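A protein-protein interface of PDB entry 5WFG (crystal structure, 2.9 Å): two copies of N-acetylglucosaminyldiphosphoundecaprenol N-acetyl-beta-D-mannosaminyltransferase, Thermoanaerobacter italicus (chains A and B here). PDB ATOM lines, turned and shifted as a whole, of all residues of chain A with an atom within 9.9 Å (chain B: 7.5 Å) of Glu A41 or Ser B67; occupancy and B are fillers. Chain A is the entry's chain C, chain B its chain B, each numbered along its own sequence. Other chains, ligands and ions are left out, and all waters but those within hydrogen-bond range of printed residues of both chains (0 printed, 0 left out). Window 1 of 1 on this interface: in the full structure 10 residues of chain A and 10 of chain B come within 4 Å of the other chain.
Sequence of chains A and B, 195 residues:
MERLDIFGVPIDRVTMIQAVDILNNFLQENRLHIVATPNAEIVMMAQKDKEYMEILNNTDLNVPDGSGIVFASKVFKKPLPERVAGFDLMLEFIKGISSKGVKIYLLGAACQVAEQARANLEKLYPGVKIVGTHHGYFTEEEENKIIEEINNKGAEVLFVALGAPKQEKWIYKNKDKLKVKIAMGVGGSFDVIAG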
ATOM      1  N   ILE A   6       9.476 -13.161 -35.898  1.00  0.00           N
ATOM      2  CA  ILE A   6       9.353 -12.517 -34.586  1.00  0.00           C
ATOM      3  C   ILE A   6      10.718 -11.897 -34.261  1.00  0.00           C
ATOM      4  O   ILE A   6      11.663 -12.629 -33.952  1.00  0.00           O
ATOM      5  CB  ILE A   6       8.885 -13.519 -33.472  1.00  0.00           C
ATOM      6  CG1 ILE A   6       7.614 -14.344 -33.882  1.00  0.00           C
ATOM      7  CG2 ILE A   6       8.714 -12.824 -32.117  1.00  0.00           C
ATOM      8  CD1 ILE A   6       6.207 -13.668 -33.836  1.00  0.00           C
ATOM      9  N   VAL A   9      14.000 -13.378 -35.692  1.00  0.00           N
ATOM     10  CA  VAL A   9      14.070 -14.831 -35.527  1.00  0.00           C
ATOM     11  C   VAL A   9      12.881 -15.483 -36.269  1.00  0.00           C
ATOM     12  O   VAL A   9      11.731 -15.144 -35.962  1.00  0.00           O
ATOM     13  CB  VAL A   9      14.111 -15.248 -34.022  1.00  0.00           C
ATOM     14  CG1 VAL A   9      14.155 -16.762 -33.855  1.00  0.00           C
ATOM     15  CG2 VAL A   9      15.280 -14.601 -33.294  1.00  0.00           C
ATOM     16  N   THR A  37      14.316 -24.391 -30.127  1.00  0.00           N
ATOM     17  CA  THR A  37      13.025 -24.052 -29.531  1.00  0.00           C
ATOM     18  C   THR A  37      13.057 -22.594 -29.022  1.00  0.00           C
ATOM     19  O   THR A  37      13.147 -22.401 -27.801  1.00  0.00           O
ATOM     20  CB  THR A  37      12.644 -25.085 -28.458  1.00  0.00           C
ATOM     21  OG1 THR A  37      13.621 -25.047 -27.423  1.00  0.00           O
ATOM     22  CG2 THR A  37      12.531 -26.495 -29.011  1.00  0.00           C
ATOM     23  N   PRO A  38      13.007 -21.553 -29.911  1.00  0.00           N
ATOM     24  CA  PRO A  38      13.081 -20.174 -29.419  1.00  0.00           C
ATOM     25  C   PRO A  38      11.937 -19.766 -28.504  1.00  0.00           C
ATOM     26  O   PRO A  38      10.821 -20.262 -28.653  1.00  0.00           O
ATOM     27  CB  PRO A  38      13.104 -19.336 -30.703  1.00  0.00           C
ATOM     28  CG  PRO A  38      13.593 -20.258 -31.743  1.00  0.00           C
ATOM     29  CD  PRO A  38      12.944 -21.559 -31.383  1.00  0.00           C
ATOM     30  N   ASN A  39      12.257 -18.892 -27.528  1.00  0.00           N
ATOM     31  CA  ASN A  39      11.362 -18.273 -26.551  1.00  0.00           C
ATOM     32  C   ASN A  39      11.727 -16.780 -26.468  1.00  0.00           C
ATOM     33  O   ASN A  39      12.589 -16.341 -27.233  1.00  0.00           O
ATOM     34  CB  ASN A  39      11.432 -18.981 -25.198  1.00  0.00           C
ATOM     35  CG  ASN A  39      12.753 -18.923 -24.480  1.00  0.00           C
ATOM     36  OD1 ASN A  39      13.712 -18.262 -24.890  1.00  0.00           O
ATOM     37  ND2 ASN A  39      12.808 -19.603 -23.353  1.00  0.00           N
ATOM     38  N   ALA A  40      11.086 -15.997 -25.577  1.00  0.00           N
ATOM     39  CA  ALA A  40      11.371 -14.561 -25.430  1.00  0.00           C
ATOM     40  C   ALA A  40      12.846 -14.288 -25.051  1.00  0.00           C
ATOM     41  O   ALA A  40      13.434 -13.353 -25.592  1.00  0.00           O
ATOM     42  CB  ALA A  40      10.423 -13.928 -24.415  1.00  0.00           C
ATOM     43  N   GLU A  41      13.440 -15.123 -24.160  1.00  0.00           N
ATOM     44  CA  GLU A  41      14.845 -15.010 -23.751  1.00  0.00           C
ATOM     45  C   GLU A  41      15.768 -15.233 -24.953  1.00  0.00           C
ATOM     46  O   GLU A  41      16.685 -14.434 -25.157  1.00  0.00           O
ATOM     47  CB  GLU A  41      15.181 -15.996 -22.620  1.00  0.00           C
ATOM     48  N   ILE A  42      15.488 -16.286 -25.773  1.00  0.00           N
ATOM     49  CA  ILE A  42      16.243 -16.615 -26.988  1.00  0.00           C
ATOM     50  C   ILE A  42      16.141 -15.493 -28.036  1.00  0.00           C
ATOM     51  O   ILE A  42      17.168 -15.057 -28.558  1.00  0.00           O
ATOM     52  CB  ILE A  42      15.863 -18.014 -27.554  1.00  0.00           C
ATOM     53  CG1 ILE A  42      16.493 -19.120 -26.708  1.00  0.00           C
ATOM     54  CG2 ILE A  42      16.273 -18.167 -29.032  1.00  0.00           C
ATOM     55  CD1 ILE A  42      15.941 -20.489 -26.930  1.00  0.00           C
ATOM     56  N   VAL A  43      14.917 -15.024 -28.328  1.00  0.00           N
ATOM     57  CA  VAL A  43      14.649 -13.961 -29.296  1.00  0.00           C
ATOM     58  C   VAL A  43      15.361 -12.643 -28.874  1.00  0.00           C
ATOM     59  O   VAL A  43      15.916 -11.948 -29.731  1.00  0.00           O
ATOM     60  CB  VAL A  43      13.124 -13.818 -29.568  1.00  0.00           C
ATOM     61  CG1 VAL A  43      12.772 -12.498 -30.248  1.00  0.00           C
ATOM     62  CG2 VAL A  43      12.621 -14.992 -30.405  1.00  0.00           C
ATOM     63  N   MET A  44      15.415 -12.356 -27.565  1.00  0.00           N
ATOM     64  CA  MET A  44      16.088 -11.181 -27.021  1.00  0.00           C
ATOM     65  C   MET A  44      17.618 -11.322 -27.136  1.00  0.00           C
ATOM     66  O   MET A  44      18.294 -10.349 -27.461  1.00  0.00           O
ATOM     67  CB  MET A  44      15.652 -10.968 -25.569  1.00  0.00           C
ATOM     68  CG  MET A  44      15.016  -9.632 -25.293  1.00  0.00           C
ATOM     69  SD  MET A  44      13.090  -9.623 -25.339  1.00  0.00           S
ATOM     70  CE  MET A  44      12.782  -8.414 -23.871  1.00  0.00           C
ATOM     71  N   MET A  45      18.152 -12.543 -26.900  1.00  0.00           N
ATOM     72  CA  MET A  45      19.579 -12.879 -27.022  1.00  0.00           C
ATOM     73  C   MET A  45      20.063 -12.616 -28.438  1.00  0.00           C
ATOM     74  O   MET A  45      21.189 -12.162 -28.615  1.00  0.00           O
ATOM     75  CB  MET A  45      19.796 -14.364 -26.711  1.00  0.00           C
ATOM     76  CG  MET A  45      20.520 -14.640 -25.427  1.00  0.00           C
ATOM     77  SD  MET A  45      20.157 -16.489 -24.919  1.00  0.00           S
ATOM     78  CE  MET A  45      19.586 -16.164 -23.047  1.00  0.00           C
ATOM     79  N   ALA A  46      19.199 -12.927 -29.437  1.00  0.00           N
ATOM     80  CA  ALA A  46      19.436 -12.778 -30.878  1.00  0.00           C
ATOM     81  C   ALA A  46      19.595 -11.320 -31.313  1.00  0.00           C
ATOM     82  O   ALA A  46      20.306 -11.061 -32.284  1.00  0.00           O
ATOM     83  CB  ALA A  46      18.323 -13.445 -31.664  1.00  0.00           C
ATOM     84  N   GLN A  47      18.956 -10.374 -30.588  1.00  0.00           N
ATOM     85  CA  GLN A  47      19.031  -8.930 -30.864  1.00  0.00           C
ATOM     86  C   GLN A  47      20.463  -8.396 -30.739  1.00  0.00           C
ATOM     87  O   GLN A  47      20.944  -7.721 -31.641  1.00  0.00           O
ATOM     88  CB  GLN A  47      18.083  -8.120 -29.951  1.00  0.00           C
ATOM     89  CG  GLN A  47      16.639  -8.615 -29.900  1.00  0.00           C
ATOM     90  CD  GLN A  47      16.017  -8.722 -31.278  1.00  0.00           C
ATOM     91  OE1 GLN A  47      15.733  -7.716 -31.955  1.00  0.00           O
ATOM     92  NE2 GLN A  47      15.811  -9.956 -31.726  1.00  0.00           N
ATOM     93  N   LYS A  48      21.142  -8.708 -29.638  1.00  0.00           N
ATOM     94  CA  LYS A  48      22.510  -8.250 -29.424  1.00  0.00           C
ATOM     95  C   LYS A  48      23.551  -9.204 -30.041  1.00  0.00           C
ATOM     96  O   LYS A  48      24.632  -8.751 -30.417  1.00  0.00           O
ATOM     97  CB  LYS A  48      22.784  -8.006 -27.932  1.00  0.00           C
ATOM     98  N   ASP A  49      23.231 -10.504 -30.157  1.00  0.00           N
ATOM     99  CA  ASP A  49      24.149 -11.488 -30.725  1.00  0.00           C
ATOM    100  C   ASP A  49      23.829 -11.797 -32.186  1.00  0.00           C
ATOM    101  O   ASP A  49      22.943 -12.609 -32.477  1.00  0.00           O
ATOM    102  CB  ASP A  49      24.188 -12.768 -29.868  1.00  0.00           C
ATOM    103  CG  ASP A  49      25.357 -13.704 -30.121  1.00  0.00           C
ATOM    104  OD1 ASP A  49      26.037 -13.549 -31.171  1.00  0.00           O
ATOM    105  OD2 ASP A  49      25.580 -14.604 -29.283  1.00  0.00           O
ATOM    106  N   TYR A  52      24.324 -15.529 -33.176  1.00  0.00           N
ATOM    107  CA  TYR A  52      23.184 -16.311 -32.691  1.00  0.00           C
ATOM    108  C   TYR A  52      21.952 -16.117 -33.583  1.00  0.00           C
ATOM    109  O   TYR A  52      21.281 -17.097 -33.914  1.00  0.00           O
ATOM    110  CB  TYR A  52      22.881 -15.983 -31.214  1.00  0.00           C
ATOM    111  CG  TYR A  52      21.896 -16.904 -30.522  1.00  0.00           C
ATOM    112  CD1 TYR A  52      21.861 -18.269 -30.809  1.00  0.00           C
ATOM    113  CD2 TYR A  52      21.048 -16.427 -29.531  1.00  0.00           C
ATOM    114  CE1 TYR A  52      20.968 -19.125 -30.161  1.00  0.00           C
ATOM    115  CE2 TYR A  52      20.160 -17.275 -28.866  1.00  0.00           C
ATOM    116  CZ  TYR A  52      20.128 -18.627 -29.179  1.00  0.00           C
ATOM    117  OH  TYR A  52      19.264 -19.472 -28.513  1.00  0.00           O
ATOM    118  N   LEU A  56      19.970 -19.031 -35.875  1.00  0.00           N
ATOM    119  CA  LEU A  56      18.514 -19.228 -35.786  1.00  0.00           C
ATOM    120  C   LEU A  56      17.796 -19.011 -37.138  1.00  0.00           C
ATOM    121  O   LEU A  56      16.703 -19.536 -37.360  1.00  0.00           O
ATOM    122  CB  LEU A  56      17.898 -18.371 -34.665  1.00  0.00           C
ATOM    123  CG  LEU A  56      18.312 -18.733 -33.239  1.00  0.00           C
ATOM    124  CD1 LEU A  56      18.151 -17.555 -32.298  1.00  0.00           C
ATOM    125  CD2 LEU A  56      17.574 -19.976 -32.731  1.00  0.00           C
ATOM    126  N   ASP A  65       8.539 -22.376 -28.393  1.00  0.00           N
ATOM    127  CA  ASP A  65       8.559 -22.684 -26.965  1.00  0.00           C
ATOM    128  C   ASP A  65       8.273 -21.369 -26.233  1.00  0.00           C
ATOM    129  O   ASP A  65       8.765 -20.318 -26.631  1.00  0.00           O
ATOM    130  CB  ASP A  65       9.941 -23.200 -26.569  1.00  0.00           C
ATOM    131  CG  ASP A  65      10.095 -23.453 -25.093  1.00  0.00           C
ATOM    132  OD1 ASP A  65       9.796 -24.576 -24.654  1.00  0.00           O
ATOM    133  OD2 ASP A  65      10.516 -22.523 -24.374  1.00  0.00           O
ATOM    134  N   GLY A  66       7.475 -21.417 -25.186  1.00  0.00           N
ATOM    135  CA  GLY A  66       7.182 -20.204 -24.437  1.00  0.00           C
ATOM    136  C   GLY A  66       6.044 -19.365 -24.989  1.00  0.00           C
ATOM    137  O   GLY A  66       6.026 -18.971 -26.171  1.00  0.00           O
ATOM    138  N   SER A  67       5.104 -19.054 -24.084  1.00  0.00           N
ATOM    139  CA  SER A  67       3.886 -18.307 -24.332  1.00  0.00           C
ATOM    140  C   SER A  67       4.098 -16.858 -24.754  1.00  0.00           C
ATOM    141  O   SER A  67       3.174 -16.272 -25.312  1.00  0.00           O
ATOM    142  CB  SER A  67       2.973 -18.392 -23.121  1.00  0.00           C
ATOM    143  OG  SER A  67       2.286 -19.625 -23.192  1.00  0.00           O
ATOM    144  N   GLY A  68       5.289 -16.309 -24.509  1.00  0.00           N
ATOM    145  CA  GLY A  68       5.633 -14.941 -24.876  1.00  0.00           C
ATOM    146  C   GLY A  68       5.535 -14.727 -26.376  1.00  0.00           C
ATOM    147  O   GLY A  68       4.782 -13.860 -26.838  1.00  0.00           O
ATOM    148  N   ILE A  69       6.266 -15.563 -27.142  1.00  0.00           N
ATOM    149  CA  ILE A  69       6.292 -15.545 -28.603  1.00  0.00           C
ATOM    150  C   ILE A  69       4.873 -15.755 -29.154  1.00  0.00           C
ATOM    151  O   ILE A  69       4.435 -14.995 -30.021  1.00  0.00           O
ATOM    152  CB  ILE A  69       7.285 -16.600 -29.154  1.00  0.00           C
ATOM    153  CG1 ILE A  69       8.742 -16.216 -28.840  1.00  0.00           C
ATOM    154  CG2 ILE A  69       7.077 -16.814 -30.667  1.00  0.00           C
ATOM    155  CD1 ILE A  69       9.742 -17.134 -29.455  1.00  0.00           C
ATOM    156  N   GLY A 163      22.484 -25.292 -22.840  1.00  0.00           N
ATOM    157  CA  GLY A 163      21.797 -24.031 -22.591  1.00  0.00           C
ATOM    158  C   GLY A 163      21.896 -23.094 -23.787  1.00  0.00           C
ATOM    159  O   GLY A 163      22.805 -23.237 -24.608  1.00  0.00           O
ATOM    160  N   ALA A 164      20.952 -22.137 -23.919  1.00  0.00           N
ATOM    161  CA  ALA A 164      20.991 -21.173 -25.018  1.00  0.00           C
ATOM    162  C   ALA A 164      21.936 -20.005 -24.648  1.00  0.00           C
ATOM    163  O   ALA A 164      21.913 -19.567 -23.489  1.00  0.00           O
ATOM    164  CB  ALA A 164      19.595 -20.652 -25.308  1.00  0.00           C
ATOM    165  N   PRO A 165      22.779 -19.480 -25.576  1.00  0.00           N
ATOM    166  CA  PRO A 165      22.943 -19.838 -26.989  1.00  0.00           C
ATOM    167  C   PRO A 165      23.981 -20.942 -27.229  1.00  0.00           C
ATOM    168  O   PRO A 165      24.154 -21.364 -28.374  1.00  0.00           O
ATOM    169  CB  PRO A 165      23.398 -18.511 -27.595  1.00  0.00           C
ATOM    170  CG  PRO A 165      24.231 -17.882 -26.528  1.00  0.00           C
ATOM    171  CD  PRO A 165      23.659 -18.348 -25.214  1.00  0.00           C
ATOM    172  N   GLU A 168      22.965 -24.145 -29.479  1.00  0.00           N
ATOM    173  CA  GLU A 168      22.804 -23.793 -30.907  1.00  0.00           C
ATOM    174  C   GLU A 168      24.156 -23.484 -31.542  1.00  0.00           C
ATOM    175  O   GLU A 168      24.423 -23.955 -32.642  1.00  0.00           O
ATOM    176  CB  GLU A 168      21.849 -22.607 -31.094  1.00  0.00           C
ATOM    177  CG  GLU A 168      20.391 -22.918 -30.775  1.00  0.00           C
ATOM    178  CD  GLU A 168      19.975 -22.870 -29.314  1.00  0.00           C
ATOM    179  OE1 GLU A 168      20.468 -21.986 -28.574  1.00  0.00           O
ATOM    180  OE2 GLU A 168      19.123 -23.700 -28.921  1.00  0.00           O
ATOM    181  N   PRO B  38      21.457  -8.530 -11.811  1.00  0.00           N
ATOM    182  CA  PRO B  38      20.057  -8.235 -12.117  1.00  0.00           C
ATOM    183  C   PRO B  38      19.613  -8.654 -13.510  1.00  0.00           C
ATOM    184  O   PRO B  38      20.414  -8.664 -14.438  1.00  0.00           O
ATOM    185  CB  PRO B  38      19.966  -6.721 -11.918  1.00  0.00           C
ATOM    186  CG  PRO B  38      21.094  -6.377 -11.043  1.00  0.00           C
ATOM    187  CD  PRO B  38      22.182  -7.280 -11.513  1.00  0.00           C
ATOM    188  N   ASN B  39      18.330  -9.039 -13.619  1.00  0.00           N
ATOM    189  CA  ASN B  39      17.610  -9.443 -14.827  1.00  0.00           C
ATOM    190  C   ASN B  39      16.234  -8.785 -14.773  1.00  0.00           C
ATOM    191  O   ASN B  39      15.996  -8.008 -13.845  1.00  0.00           O
ATOM    192  CB  ASN B  39      17.529 -10.974 -14.955  1.00  0.00           C
ATOM    193  CG  ASN B  39      16.754 -11.709 -13.886  1.00  0.00           C
ATOM    194  OD1 ASN B  39      16.118 -11.131 -13.003  1.00  0.00           O
ATOM    195  ND2 ASN B  39      16.781 -13.025 -13.951  1.00  0.00           N
ATOM    196  N   ALA B  40      15.336  -9.056 -15.755  1.00  0.00           N
ATOM    197  CA  ALA B  40      13.984  -8.451 -15.780  1.00  0.00           C
ATOM    198  C   ALA B  40      13.165  -8.791 -14.527  1.00  0.00           C
ATOM    199  O   ALA B  40      12.520  -7.899 -13.989  1.00  0.00           O
ATOM    200  CB  ALA B  40      13.229  -8.842 -17.042  1.00  0.00           C
ATOM    201  N   PRO B  64      24.928  -7.313 -16.132  1.00  0.00           N
ATOM    202  CA  PRO B  64      23.712  -7.487 -16.951  1.00  0.00           C
ATOM    203  C   PRO B  64      23.301  -8.943 -17.267  1.00  0.00           C
ATOM    204  O   PRO B  64      23.416  -9.349 -18.427  1.00  0.00           O
ATOM    205  CB  PRO B  64      24.022  -6.685 -18.226  1.00  0.00           C
ATOM    206  CG  PRO B  64      25.300  -5.945 -17.951  1.00  0.00           C
ATOM    207  CD  PRO B  64      26.022  -6.710 -16.913  1.00  0.00           C
ATOM    208  N   ASP B  65      22.761  -9.712 -16.275  1.00  0.00           N
ATOM    209  CA  ASP B  65      22.285 -11.081 -16.532  1.00  0.00           C
ATOM    210  C   ASP B  65      20.932 -10.983 -17.246  1.00  0.00           C
ATOM    211  O   ASP B  65      20.117 -10.115 -16.899  1.00  0.00           O
ATOM    212  CB  ASP B  65      22.118 -11.852 -15.214  1.00  0.00           C
ATOM    213  CG  ASP B  65      21.573 -13.255 -15.364  1.00  0.00           C
ATOM    214  OD1 ASP B  65      20.347 -13.416 -15.349  1.00  0.00           O
ATOM    215  OD2 ASP B  65      22.373 -14.188 -15.480  1.00  0.00           O
ATOM    216  N   GLY B  66      20.686 -11.829 -18.238  1.00  0.00           N
ATOM    217  CA  GLY B  66      19.395 -11.749 -18.918  1.00  0.00           C
ATOM    218  C   GLY B  66      19.281 -10.716 -20.038  1.00  0.00           C
ATOM    219  O   GLY B  66      19.535  -9.516 -19.854  1.00  0.00           O
ATOM    220  N   SER B  67      18.857 -11.214 -21.208  1.00  0.00           N
ATOM    221  CA  SER B  67      18.703 -10.524 -22.464  1.00  0.00           C
ATOM    222  C   SER B  67      17.710  -9.383 -22.469  1.00  0.00           C
ATOM    223  O   SER B  67      17.810  -8.508 -23.332  1.00  0.00           O
ATOM    224  CB  SER B  67      18.346 -11.532 -23.545  1.00  0.00           C
ATOM    225  OG  SER B  67      19.485 -12.292 -23.894  1.00  0.00           O
ATOM    226  N   GLY B  68      16.754  -9.408 -21.539  1.00  0.00           N
ATOM    227  CA  GLY B  68      15.722  -8.391 -21.399  1.00  0.00           C
ATOM    228  C   GLY B  68      16.319  -7.026 -21.153  1.00  0.00           C
ATOM    229  O   GLY B  68      16.073  -6.100 -21.933  1.00  0.00           O
ATOM    230  N   ILE B  69      17.143  -6.916 -20.088  1.00  0.00           N
ATOM    231  CA  ILE B  69      17.836  -5.683 -19.706  1.00  0.00           C
ATOM    232  C   ILE B  69      18.706  -5.169 -20.859  1.00  0.00           C
ATOM    233  O   ILE B  69      18.631  -3.988 -21.210  1.00  0.00           O
ATOM    234  CB  ILE B  69      18.643  -5.873 -18.398  1.00  0.00           C
ATOM    235  CG1 ILE B  69      17.721  -6.098 -17.163  1.00  0.00           C
ATOM    236  CG2 ILE B  69      19.625  -4.703 -18.175  1.00  0.00           C
ATOM    237  CD1 ILE B  69      18.505  -6.198 -15.857  1.00  0.00           C
ATOM    238  N   VAL B  70      19.504  -6.070 -21.460  1.00  0.00           N
ATOM    239  CA  VAL B  70      20.393  -5.766 -22.588  1.00  0.00           C
ATOM    240  C   VAL B  70      19.587  -5.251 -23.805  1.00  0.00           C
ATOM    241  O   VAL B  70      20.022  -4.288 -24.444  1.00  0.00           O
ATOM    242  CB  VAL B  70      21.339  -6.937 -22.919  1.00  0.00           C
ATOM    243  CG1 VAL B  70      22.367  -6.526 -23.957  1.00  0.00           C
ATOM    244  CG2 VAL B  70      22.043  -7.444 -21.655  1.00  0.00           C
ATOM    245  N   PHE B  71      18.384  -5.820 -24.062  1.00  0.00           N
ATOM    246  CA  PHE B  71      17.493  -5.359 -25.142  1.00  0.00           C
ATOM    247  C   PHE B  71      16.909  -3.955 -24.828  1.00  0.00           C
ATOM    248  O   PHE B  71      16.923  -3.084 -25.701  1.00  0.00           O
ATOM    249  CB  PHE B  71      16.377  -6.385 -25.429  1.00  0.00           C
ATOM    250  CG  PHE B  71      15.286  -5.935 -26.365  1.00  0.00           C
ATOM    251  CD1 PHE B  71      15.533  -5.797 -27.732  1.00  0.00           C
ATOM    252  CD2 PHE B  71      14.015  -5.641 -25.885  1.00  0.00           C
ATOM    253  CE1 PHE B  71      14.519  -5.378 -28.606  1.00  0.00           C
ATOM    254  CE2 PHE B  71      12.998  -5.232 -26.753  1.00  0.00           C
ATOM    255  CZ  PHE B  71      13.258  -5.095 -28.109  1.00  0.00           C
ATOM    256  N   ALA B  72      16.450  -3.739 -23.576  1.00  0.00           N
ATOM    257  CA  ALA B  72      15.937  -2.456 -23.095  1.00  0.00           C
ATOM    258  C   ALA B  72      16.994  -1.358 -23.215  1.00  0.00           C
ATOM    259  O   ALA B  72      16.670  -0.266 -23.669  1.00  0.00           O
ATOM    260  CB  ALA B  72      15.491  -2.580 -21.647  1.00  0.00           C
ATOM    261  N   SER B  73      18.265  -1.670 -22.865  1.00  0.00           N
ATOM    262  CA  SER B  73      19.405  -0.752 -22.939  1.00  0.00           C
ATOM    263  C   SER B  73      19.690  -0.226 -24.340  1.00  0.00           C
ATOM    264  O   SER B  73      20.248   0.861 -24.452  1.00  0.00           O
ATOM    265  CB  SER B  73      20.656  -1.390 -22.344  1.00  0.00           C
ATOM    266  OG  SER B  73      21.322  -2.229 -23.275  1.00  0.00           O
ATOM    267  N   ARG B  83      25.412  -9.622 -22.756  1.00  0.00           N
ATOM    268  CA  ARG B  83      24.808 -10.236 -21.574  1.00  0.00           C
ATOM    269  C   ARG B  83      25.966 -10.723 -20.723  1.00  0.00           C
ATOM    270  O   ARG B  83      26.955 -11.198 -21.268  1.00  0.00           O
ATOM    271  CB  ARG B  83      23.872 -11.412 -21.931  1.00  0.00           C
ATOM    272  CG  ARG B  83      24.559 -12.734 -22.308  1.00  0.00           C
ATOM    273  CD  ARG B  83      23.660 -13.949 -22.180  1.00  0.00           C
ATOM    274  NE  ARG B  83      22.714 -13.840 -21.069  1.00  0.00           N
ATOM    275  CZ  ARG B  83      22.112 -14.877 -20.499  1.00  0.00           C
ATOM    276  NH1 ARG B  83      22.368 -16.113 -20.914  1.00  0.00           N
ATOM    277  NH2 ARG B  83      21.255 -14.688 -19.505  1.00  0.00           N
ATOM    278  N   VAL B  84      25.889 -10.550 -19.417  1.00  0.00           N
ATOM    279  CA  VAL B  84      26.936 -11.069 -18.541  1.00  0.00           C
ATOM    280  C   VAL B  84      26.179 -12.044 -17.618  1.00  0.00           C
ATOM    281  O   VAL B  84      25.661 -11.629 -16.580  1.00  0.00           O
ATOM    282  CB  VAL B  84      27.759  -9.963 -17.815  1.00  0.00           C
ATOM    283  CG1 VAL B  84      28.880 -10.577 -16.979  1.00  0.00           C
ATOM    284  CG2 VAL B  84      28.327  -8.947 -18.814  1.00  0.00           C
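Hydrophobic or aromatic side chains of chain A within 4 Å of the printed part of chain B: Met A44 and Met A45. Among the printed residues, no Asp or Glu carboxylate lies within 4 Å of a Lys or Arg side-chain nitrogen of the other chain.
Among the printed residues, pairs that only touch across the chains: Met A44 with Ser B67, Met A45 with Arg B83, Met A44 with Phe B71, Glu A41 with Ser B67, Gln A47 with Phe B71 and Met A44 with Gly B68.
Glu A41 touches just one residue of chain B: Ser B67 (3.7 Å). Of chain A, only Glu A41, Met A44 and Met A45 come within 4 Å of Ser B67. No residue of chain A comes within 4 Å of Gly B66. No residue of chain A comes within 4 Å of Val B70. Printed residues of chain A within 4 Å of Arg B83: Met A45. Of the printed residues of chain B, Gln A47 touches Phe B71 (3.7 Å). Of the printed residues of chain A, Phe B71 touches Met A44 and Gln A47. Printed residues of chain B within 4 Å of Met A45: Ser B67 and Arg B83. Of the printed residues of chain B, Met A44 touches Ser B67 (3.4 Å), Gly B68 (3.8 Å) and Phe B71 (3.5 Å). Val B84 touches none of the printed residues of chain A. Ile A6 touches none of the printed residues of chain B. The nearest residue of chain B that does not touch Glu A41 is Gly B68 (6.2 Å).
Positions printed for both chains: 38, 39, 40, 65, 66, 67, 68 and 69.
N of Met A45 sits close to OG of Ser B67.
The side-chain amide oxygen (OD1) of Asn A39 is in hydrogen-bond range of the backbone NH (N) of Glu A41, 3.2 Å away. NE2 of Gln A47 sits at hydrogen-bond distance from O of Val A43, at 2.8 Å.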
